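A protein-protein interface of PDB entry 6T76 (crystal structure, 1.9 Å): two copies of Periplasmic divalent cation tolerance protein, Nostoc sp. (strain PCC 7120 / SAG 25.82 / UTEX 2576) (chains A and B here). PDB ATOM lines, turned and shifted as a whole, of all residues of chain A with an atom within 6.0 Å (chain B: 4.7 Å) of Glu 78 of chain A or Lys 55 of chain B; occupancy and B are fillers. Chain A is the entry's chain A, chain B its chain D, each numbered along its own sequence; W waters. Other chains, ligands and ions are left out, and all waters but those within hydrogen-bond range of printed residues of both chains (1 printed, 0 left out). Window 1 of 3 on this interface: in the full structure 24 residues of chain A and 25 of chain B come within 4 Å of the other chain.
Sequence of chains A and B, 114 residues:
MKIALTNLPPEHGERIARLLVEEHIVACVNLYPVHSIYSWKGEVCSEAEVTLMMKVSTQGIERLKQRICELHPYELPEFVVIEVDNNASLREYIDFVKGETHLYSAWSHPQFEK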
ATOM      1  N   LEU A   5       5.015 -31.595  21.277  1.00  0.00           N
ATOM      2  CA  LEU A   5       6.350 -32.234  21.314  1.00  0.00           C
ATOM      3  C   LEU A   5       7.121 -31.723  22.498  1.00  0.00           C
ATOM      4  O   LEU A   5       7.116 -30.496  22.780  1.00  0.00           O
ATOM      5  CB  LEU A   5       7.164 -31.852  20.072  1.00  0.00           C
ATOM      6  CG  LEU A   5       6.569 -32.239  18.705  1.00  0.00           C
ATOM      7  CD1 LEU A   5       7.406 -31.611  17.610  1.00  0.00           C
ATOM      8  CD2 LEU A   5       6.476 -33.733  18.489  1.00  0.00           C
ATOM      9  N   THR A   6       7.835 -32.614  23.166  1.00  0.00           N
ATOM     10  CA  THR A   6       8.887 -32.203  24.061  1.00  0.00           C
ATOM     11  C   THR A   6      10.071 -33.169  23.864  1.00  0.00           C
ATOM     12  O   THR A   6       9.893 -34.251  23.334  1.00  0.00           O
ATOM     13  CB  THR A   6       8.424 -32.185  25.510  1.00  0.00           C
ATOM     14  OG1 THR A   6       9.438 -31.604  26.338  1.00  0.00           O
ATOM     15  CG2 THR A   6       8.136 -33.580  26.039  1.00  0.00           C
ATOM     16  N   ASN A   7      11.263 -32.742  24.250  1.00  0.00           N
ATOM     17  CA  ASN A   7      12.458 -33.622  24.319  1.00  0.00           C
ATOM     18  C   ASN A   7      12.792 -33.810  25.767  1.00  0.00           C
ATOM     19  O   ASN A   7      12.815 -32.835  26.548  1.00  0.00           O
ATOM     20  CB  ASN A   7      13.630 -32.940  23.652  1.00  0.00           C
ATOM     21  CG  ASN A   7      13.700 -33.189  22.165  1.00  0.00           C
ATOM     22  OD1 ASN A   7      14.648 -32.756  21.520  1.00  0.00           O
ATOM     23  ND2 ASN A   7      12.769 -33.886  21.620  1.00  0.00           N
ATOM     24  N   GLU A  49      18.627 -37.643  23.587  1.00  0.00           N
ATOM     25  CA  GLU A  49      17.307 -37.343  24.149  1.00  0.00           C
ATOM     26  C   GLU A  49      16.264 -38.296  23.572  1.00  0.00           C
ATOM     27  O   GLU A  49      16.586 -39.115  22.728  1.00  0.00           O
ATOM     28  CB  GLU A  49      16.945 -35.884  23.874  1.00  0.00           C
ATOM     29  CG  GLU A  49      17.821 -34.920  24.665  1.00  0.00           C
ATOM     30  CD  GLU A  49      17.347 -33.491  24.533  1.00  0.00           C
ATOM     31  OE1 GLU A  49      17.041 -33.053  23.411  1.00  0.00           O
ATOM     32  OE2 GLU A  49      17.262 -32.823  25.557  1.00  0.00           O
ATOM     33  N   ILE A  68       3.481 -31.257  31.971  1.00  0.00           N
ATOM     34  CA  ILE A  68       4.866 -31.205  31.457  1.00  0.00           C
ATOM     35  C   ILE A  68       5.768 -30.287  32.258  1.00  0.00           C
ATOM     36  O   ILE A  68       6.881 -30.664  32.624  1.00  0.00           O
ATOM     37  CB  ILE A  68       4.925 -30.781  29.950  1.00  0.00           C
ATOM     38  CG1 ILE A  68       4.349 -31.874  29.089  1.00  0.00           C
ATOM     39  CG2 ILE A  68       6.373 -30.480  29.498  1.00  0.00           C
ATOM     40  CD1 ILE A  68       5.166 -33.158  29.118  1.00  0.00           C
ATOM     41  N   HIS A  72       9.029 -31.776  34.051  1.00  0.00           N
ATOM     42  CA  HIS A  72      10.169 -31.711  33.184  1.00  0.00           C
ATOM     43  C   HIS A  72      11.403 -31.413  33.997  1.00  0.00           C
ATOM     44  O   HIS A  72      11.399 -30.516  34.809  1.00  0.00           O
ATOM     45  CB  HIS A  72       9.992 -30.621  32.097  1.00  0.00           C
ATOM     46  CG  HIS A  72      10.699 -30.931  30.811  1.00  0.00           C
ATOM     47  ND1 HIS A  72      12.071 -30.904  30.693  1.00  0.00           N
ATOM     48  CD2 HIS A  72      10.227 -31.288  29.597  1.00  0.00           C
ATOM     49  CE1 HIS A  72      12.413 -31.215  29.457  1.00  0.00           C
ATOM     50  NE2 HIS A  72      11.313 -31.484  28.778  1.00  0.00           N
ATOM     51  N   TYR A  74      14.254 -30.067  32.932  1.00  0.00           N
ATOM     52  CA  TYR A  74      15.072 -28.978  32.430  1.00  0.00           C
ATOM     53  C   TYR A  74      14.568 -27.632  32.925  1.00  0.00           C
ATOM     54  O   TYR A  74      13.368 -27.422  33.058  1.00  0.00           O
ATOM     55  CB  TYR A  74      15.099 -28.930  30.887  1.00  0.00           C
ATOM     56  CG  TYR A  74      15.718 -30.088  30.169  1.00  0.00           C
ATOM     57  CD1 TYR A  74      16.589 -30.976  30.794  1.00  0.00           C
ATOM     58  CD2 TYR A  74      15.509 -30.235  28.809  1.00  0.00           C
ATOM     59  CE1 TYR A  74      17.138 -32.020  30.094  1.00  0.00           C
ATOM     60  CE2 TYR A  74      16.033 -31.278  28.106  1.00  0.00           C
ATOM     61  CZ  TYR A  74      16.859 -32.158  28.758  1.00  0.00           C
ATOM     62  OH  TYR A  74      17.399 -33.201  28.017  1.00  0.00           O
ATOM     63  N   LEU A  76      14.467 -25.012  31.204  1.00  0.00           N
ATOM     64  CA  LEU A  76      13.618 -24.507  30.144  1.00  0.00           C
ATOM     65  C   LEU A  76      13.141 -25.686  29.311  1.00  0.00           C
ATOM     66  O   LEU A  76      13.824 -26.108  28.422  1.00  0.00           O
ATOM     67  CB  LEU A  76      14.396 -23.513  29.305  1.00  0.00           C
ATOM     68  CG  LEU A  76      13.794 -22.883  28.052  1.00  0.00           C
ATOM     69  CD1 LEU A  76      12.314 -22.670  28.199  1.00  0.00           C
ATOM     70  CD2 LEU A  76      14.487 -21.558  27.830  1.00  0.00           C
ATOM     71  N   PRO A  77      11.945 -26.186  29.592  1.00  0.00           N
ATOM     72  CA  PRO A  77      11.477 -27.336  28.841  1.00  0.00           C
ATOM     73  C   PRO A  77      10.968 -26.949  27.461  1.00  0.00           C
ATOM     74  O   PRO A  77      10.473 -25.845  27.257  1.00  0.00           O
ATOM     75  CB  PRO A  77      10.353 -27.890  29.706  1.00  0.00           C
ATOM     76  CG  PRO A  77       9.885 -26.790  30.545  1.00  0.00           C
ATOM     77  CD  PRO A  77      11.030 -25.815  30.689  1.00  0.00           C
ATOM     78  N   GLU A  78      11.182 -27.829  26.519  1.00  0.00           N
ATOM     79  CA  GLU A  78      10.577 -27.706  25.227  1.00  0.00           C
ATOM     80  C   GLU A  78       9.103 -28.102  25.330  1.00  0.00           C
ATOM     81  O   GLU A  78       8.746 -29.135  25.897  1.00  0.00           O
ATOM     82  CB  GLU A  78      11.278 -28.618  24.228  1.00  0.00           C
ATOM     83  CG  GLU A  78      10.559 -28.666  22.887  1.00  0.00           C
ATOM     84  CD  GLU A  78      11.254 -29.564  21.871  1.00  0.00           C
ATOM     85  OE1 GLU A  78      12.225 -30.279  22.229  1.00  0.00           O
ATOM     86  OE2 GLU A  78      10.861 -29.502  20.694  1.00  0.00           O
ATOM     87  N   PHE A  79       8.218 -27.253  24.841  1.00  0.00           N
ATOM     88  CA  PHE A  79       6.833 -27.662  24.669  1.00  0.00           C
ATOM     89  C   PHE A  79       6.288 -26.928  23.475  1.00  0.00           C
ATOM     90  O   PHE A  79       6.022 -25.719  23.540  1.00  0.00           O
ATOM     91  CB  PHE A  79       6.024 -27.396  25.908  1.00  0.00           C
ATOM     92  CG  PHE A  79       4.652 -27.897  25.805  1.00  0.00           C
ATOM     93  CD1 PHE A  79       4.371 -29.241  25.996  1.00  0.00           C
ATOM     94  CD2 PHE A  79       3.611 -27.054  25.470  1.00  0.00           C
ATOM     95  CE1 PHE A  79       3.048 -29.713  25.879  1.00  0.00           C
ATOM     96  CE2 PHE A  79       2.308 -27.516  25.389  1.00  0.00           C
ATOM     97  CZ  PHE A  79       2.030 -28.834  25.575  1.00  0.00           C
ATOM     98  N   VAL A  80       6.227 -27.625  22.355  1.00  0.00           N
ATOM     99  CA  VAL A  80       5.854 -27.042  21.081  1.00  0.00           C
ATOM    100  C   VAL A  80       4.614 -27.769  20.570  1.00  0.00           C
ATOM    101  O   VAL A  80       4.585 -28.956  20.473  1.00  0.00           O
ATOM    102  CB  VAL A  80       6.961 -27.194  20.040  1.00  0.00           C
ATOM    103  CG1 VAL A  80       6.529 -26.590  18.699  1.00  0.00           C
ATOM    104  CG2 VAL A  80       8.194 -26.495  20.542  1.00  0.00           C
ATOM    105  N   MET B   1       7.475 -19.049  16.418  1.00  0.00           N
ATOM    106  CA  MET B   1       8.490 -19.979  15.890  1.00  0.00           C
ATOM    107  C   MET B   1       7.789 -20.892  14.886  1.00  0.00           C
ATOM    108  O   MET B   1       6.573 -20.960  14.865  1.00  0.00           O
ATOM    109  CB  MET B   1       9.125 -20.770  17.029  1.00  0.00           C
ATOM    110  CG  MET B   1       8.207 -21.828  17.584  1.00  0.00           C
ATOM    111  SD  MET B   1       8.976 -22.948  18.766  1.00  0.00           S
ATOM    112  CE  MET B   1       9.752 -24.088  17.637  1.00  0.00           C
ATOM    113  N   LYS B   2       8.570 -21.599  14.078  1.00  0.00           N
ATOM    114  CA  LYS B   2       8.055 -22.656  13.243  1.00  0.00           C
ATOM    115  C   LYS B   2       9.081 -23.823  13.305  1.00  0.00           C
ATOM    116  O   LYS B   2      10.125 -23.711  13.899  1.00  0.00           O
ATOM    117  CB  LYS B   2       7.828 -22.222  11.768  1.00  0.00           C
ATOM    118  CG  LYS B   2       6.599 -21.245  11.523  1.00  0.00           C
ATOM    119  CD  LYS B   2       6.171 -20.858  10.053  1.00  0.00           C
ATOM    120  N   ILE B   3       8.668 -24.964  12.796  1.00  0.00           N
ATOM    121  CA  ILE B   3       9.517 -26.156  12.647  1.00  0.00           C
ATOM    122  C   ILE B   3       9.776 -26.348  11.167  1.00  0.00           C
ATOM    123  O   ILE B   3       8.836 -26.256  10.354  1.00  0.00           O
ATOM    124  CB  ILE B   3       8.852 -27.380  13.297  1.00  0.00           C
ATOM    125  CG1 ILE B   3       8.933 -27.233  14.820  1.00  0.00           C
ATOM    126  CG2 ILE B   3       9.576 -28.685  12.904  1.00  0.00           C
ATOM    127  CD1 ILE B   3       8.067 -28.234  15.564  1.00  0.00           C
ATOM    128  N   VAL B  26      19.488 -21.570  13.458  1.00  0.00           N
ATOM    129  CA  VAL B  26      18.396 -22.249  14.171  1.00  0.00           C
ATOM    130  C   VAL B  26      18.831 -22.310  15.610  1.00  0.00           C
ATOM    131  O   VAL B  26      20.050 -22.195  15.924  1.00  0.00           O
ATOM    132  CB  VAL B  26      18.120 -23.685  13.662  1.00  0.00           C
ATOM    133  CG1 VAL B  26      17.841 -23.712  12.162  1.00  0.00           C
ATOM    134  CG2 VAL B  26      19.287 -24.619  13.993  1.00  0.00           C
ATOM    135  N   ALA B  27      17.858 -22.499  16.487  1.00  0.00           N
ATOM    136  CA  ALA B  27      18.111 -22.587  17.887  1.00  0.00           C
ATOM    137  C   ALA B  27      18.485 -24.041  18.289  1.00  0.00           C
ATOM    138  O   ALA B  27      19.246 -24.222  19.198  1.00  0.00           O
ATOM    139  CB  ALA B  27      16.862 -22.144  18.637  1.00  0.00           C
ATOM    140  N   CYS B  28      17.915 -25.014  17.593  1.00  0.00           N
ATOM    141  CA  CYS B  28      17.906 -26.427  18.010  1.00  0.00           C
ATOM    142  C   CYS B  28      17.650 -27.263  16.772  1.00  0.00           C
ATOM    143  O   CYS B  28      16.790 -26.900  15.944  1.00  0.00           O
ATOM    144  CB  CYS B  28      16.846 -26.671  19.089  1.00  0.00           C
ATOM    145  SG  CYS B  28      16.693 -28.463  19.475  1.00  0.00           S
ATOM    146  N   ASN B  30      16.886 -31.461  15.969  1.00  0.00           N
ATOM    147  CA  ASN B  30      16.734 -32.837  16.374  1.00  0.00           C
ATOM    148  C   ASN B  30      16.968 -33.730  15.167  1.00  0.00           C
ATOM    149  O   ASN B  30      16.382 -33.501  14.155  1.00  0.00           O
ATOM    150  CB  ASN B  30      15.389 -33.158  16.902  1.00  0.00           C
ATOM    151  CG  ASN B  30      15.012 -32.340  18.131  1.00  0.00           C
ATOM    152  OD1 ASN B  30      13.881 -31.815  18.192  1.00  0.00           O
ATOM    153  ND2 ASN B  30      15.898 -32.179  19.049  1.00  0.00           N
ATOM    154  N   MET B  53      14.919 -32.028  12.203  1.00  0.00           N
ATOM    155  CA  MET B  53      13.788 -31.221  12.659  1.00  0.00           C
ATOM    156  C   MET B  53      14.327 -29.946  13.347  1.00  0.00           C
ATOM    157  O   MET B  53      14.991 -30.007  14.383  1.00  0.00           O
ATOM    158  CB  MET B  53      12.897 -32.017  13.603  1.00  0.00           C
ATOM    159  CG  MET B  53      11.929 -31.112  14.395  1.00  0.00           C
ATOM    160  SD  MET B  53      10.654 -32.070  15.199  1.00  0.00           S
ATOM    161  CE  MET B  53      11.337 -32.464  16.814  1.00  0.00           C
ATOM    162  N   MET B  54      14.145 -28.806  12.685  1.00  0.00           N
ATOM    163  CA  MET B  54      14.837 -27.553  13.020  1.00  0.00           C
ATOM    164  C   MET B  54      13.850 -26.599  13.636  1.00  0.00           C
ATOM    165  O   MET B  54      12.804 -26.344  13.066  1.00  0.00           O
ATOM    166  CB  MET B  54      15.439 -26.983  11.746  1.00  0.00           C
ATOM    167  CG  MET B  54      16.523 -27.897  11.136  1.00  0.00           C
ATOM    168  SD  MET B  54      16.997 -27.528   9.472  1.00  0.00           S
ATOM    169  CE  MET B  54      15.611 -28.081   8.492  1.00  0.00           C
ATOM    170  N   LYS B  55      14.168 -26.082  14.805  1.00  0.00           N
ATOM    171  CA  LYS B  55      13.334 -25.087  15.472  1.00  0.00           C
ATOM    172  C   LYS B  55      13.930 -23.700  15.285  1.00  0.00           C
ATOM    173  O   LYS B  55      15.126 -23.455  15.592  1.00  0.00           O
ATOM    174  CB  LYS B  55      13.225 -25.421  16.952  1.00  0.00           C
ATOM    175  CG  LYS B  55      12.443 -26.708  17.096  1.00  0.00           C
ATOM    176  CD  LYS B  55      12.879 -27.467  18.310  1.00  0.00           C
ATOM    177  CE  LYS B  55      12.733 -28.948  18.036  1.00  0.00           C
ATOM    178  NZ  LYS B  55      13.477 -29.660  19.086  1.00  0.00           N
ATOM    179  N   VAL B  56      13.119 -22.812  14.726  1.00  0.00           N
ATOM    180  CA  VAL B  56      13.619 -21.534  14.279  1.00  0.00           C
ATOM    181  C   VAL B  56      12.522 -20.470  14.470  1.00  0.00           C
ATOM    182  O   VAL B  56      11.359 -20.796  14.460  1.00  0.00           O
ATOM    183  CB  VAL B  56      14.078 -21.647  12.797  1.00  0.00           C
ATOM    184  CG1 VAL B  56      12.931 -22.015  11.889  1.00  0.00           C
ATOM    185  CG2 VAL B  56      14.753 -20.355  12.331  1.00  0.00           C
ATOM    186  N   SER B  57      12.914 -19.241  14.722  1.00  0.00           N
ATOM    187  CA  SER B  57      11.955 -18.141  14.771  1.00  0.00           C
ATOM    188  C   SER B  57      11.231 -18.041  13.453  1.00  0.00           C
ATOM    189  O   SER B  57      11.743 -18.415  12.377  1.00  0.00           O
ATOM    190  CB  SER B  57      12.652 -16.825  15.070  1.00  0.00           C
ATOM    191  OG  SER B  57      13.495 -16.432  14.027  1.00  0.00           O
ATOM    192  N   TYR B  93       9.636 -21.012  25.954  1.00  0.00           N
ATOM    193  CA  TYR B  93      10.364 -21.777  24.946  1.00  0.00           C
ATOM    194  C   TYR B  93      10.417 -21.058  23.574  1.00  0.00           C
ATOM    195  O   TYR B  93      11.458 -21.013  22.922  1.00  0.00           O
ATOM    196  CB  TYR B  93       9.833 -23.206  24.788  1.00  0.00           C
ATOM    197  CG  TYR B  93      10.727 -23.984  23.872  1.00  0.00           C
ATOM    198  CD1 TYR B  93      11.972 -24.472  24.328  1.00  0.00           C
ATOM    199  CD2 TYR B  93      10.366 -24.237  22.560  1.00  0.00           C
ATOM    200  CE1 TYR B  93      12.800 -25.181  23.471  1.00  0.00           C
ATOM    201  CE2 TYR B  93      11.203 -24.937  21.689  1.00  0.00           C
ATOM    202  CZ  TYR B  93      12.413 -25.412  22.146  1.00  0.00           C
ATOM    203  OH  TYR B  93      13.220 -26.110  21.276  1.00  0.00           O
ATOM    204  N   VAL B  97      13.695 -19.715  21.486  1.00  0.00           N
ATOM    205  CA  VAL B  97      13.975 -20.017  20.086  1.00  0.00           C
ATOM    206  C   VAL B  97      14.200 -18.728  19.327  1.00  0.00           C
ATOM    207  O   VAL B  97      15.145 -18.648  18.516  1.00  0.00           O
ATOM    208  CB  VAL B  97      12.838 -20.843  19.459  1.00  0.00           C
ATOM    209  CG1 VAL B  97      12.959 -20.873  17.941  1.00  0.00           C
ATOM    210  CG2 VAL B  97      12.873 -22.265  20.008  1.00  0.00           C
HETATM  211  O   HOH W   1      10.999 -32.322  20.076  1.00  0.00           O
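Water W1 lies within hydrogen-bond range of the side-chain amide nitrogen (ND2) of Asn 7 of chain A (2.8 Å), the side-chain carboxylate (OE2) of Glu 78 of chain A (2.9 Å) and the side-chain amide oxygen (OD1) of Asn 30 of chain B (3.5 Å).
Of the printed residues of chain B, Leu 76 of chain A touches Tyr 93 (3.9 Å).
Of the printed residues of chain B, Pro 77 of chain A touches Tyr 93 (3.6 Å).
Printed residues of chain B within 4 Å of Val 80 of chain A: Ile 3 (3.9 Å) and Tyr 93 (3.6 Å).
Printed residues of chain A within 4 Å of Ile 3 of chain B: Val 80 (3.9 Å).
Lys 55 of chain B touches one residue of chain A.
The nearest residue of chain B that does not touch Glu 78 of chain A is Asn 30 of chain B (4.6 Å).
The nearest printed residue of chain A that does not touch Tyr 93 of chain B is Phe 79 of chain A (4.2 Å).
No position is printed for both chains.
O of Glu 78 of chain A sits at hydrogen-bond distance from OG1 of Thr 6 of chain A (2.6 Å).
The side-chain carboxylate (OE1) of Glu 49 of chain A sits close to the side-chain amide oxygen (OD1) of Asn 7 of chain A (3.1 Å).
NE2 of His 72 of chain A is in hydrogen-bond range of O of Asn 7 of chain A (3.0 Å).
The backbone NH (N) of Asn 7 of chain A sits close to the side-chain carboxylate (OE1) of Glu 78 of chain A, at 3.3 Å.
The backbone NH (N) of Ala 27 of chain B lies within hydrogen-bond range of the backbone carbonyl oxygen (O) of Lys 55 of chain B.
The side-chain amino group (NZ) of Lys 55 of chain B sits close to the side-chain amide nitrogen (ND2) of Asn 30 of chain B.
Of the 14 printed residues of chain B, 4 touch a printed residue of chain A.
Printed residues of chain B that touch a printed residue of chain A: Ile 3, Asn 30, Lys 55 and Tyr 93.
Among the printed residues, 7 pairs touch across the chains.
Among the printed residues, Asp or Glu carboxylates within 4 Å of a Lys or Arg side-chain nitrogen of the other chain: Glu 78 of chain A with Lys 55 of chain B.
Among the printed residues, pairs that only touch across the chains: Pro 77 of chain A with Tyr 93 of chain B (3.6 Å), Val 80 of chain A with Tyr 93 of chain B (3.6 Å), Glu 78 of chain A with Tyr 93 of chain B (3.6 Å), Val 80 of chain A with Ile 3 of chain B (3.9 Å) and Leu 76 of chain A with Tyr 93 of chain B (3.9 Å).
OD1 of Asn 7 of chain A sits at hydrogen-bond distance from ND2 of Asn 30 of chain B (2.8 Å).
The side-chain carboxylate (OE2) of Glu 78 of chain A lies within salt-bridge range of the side-chain amino group (NZ) of Lys 55 of chain B, 3.1 Å away.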
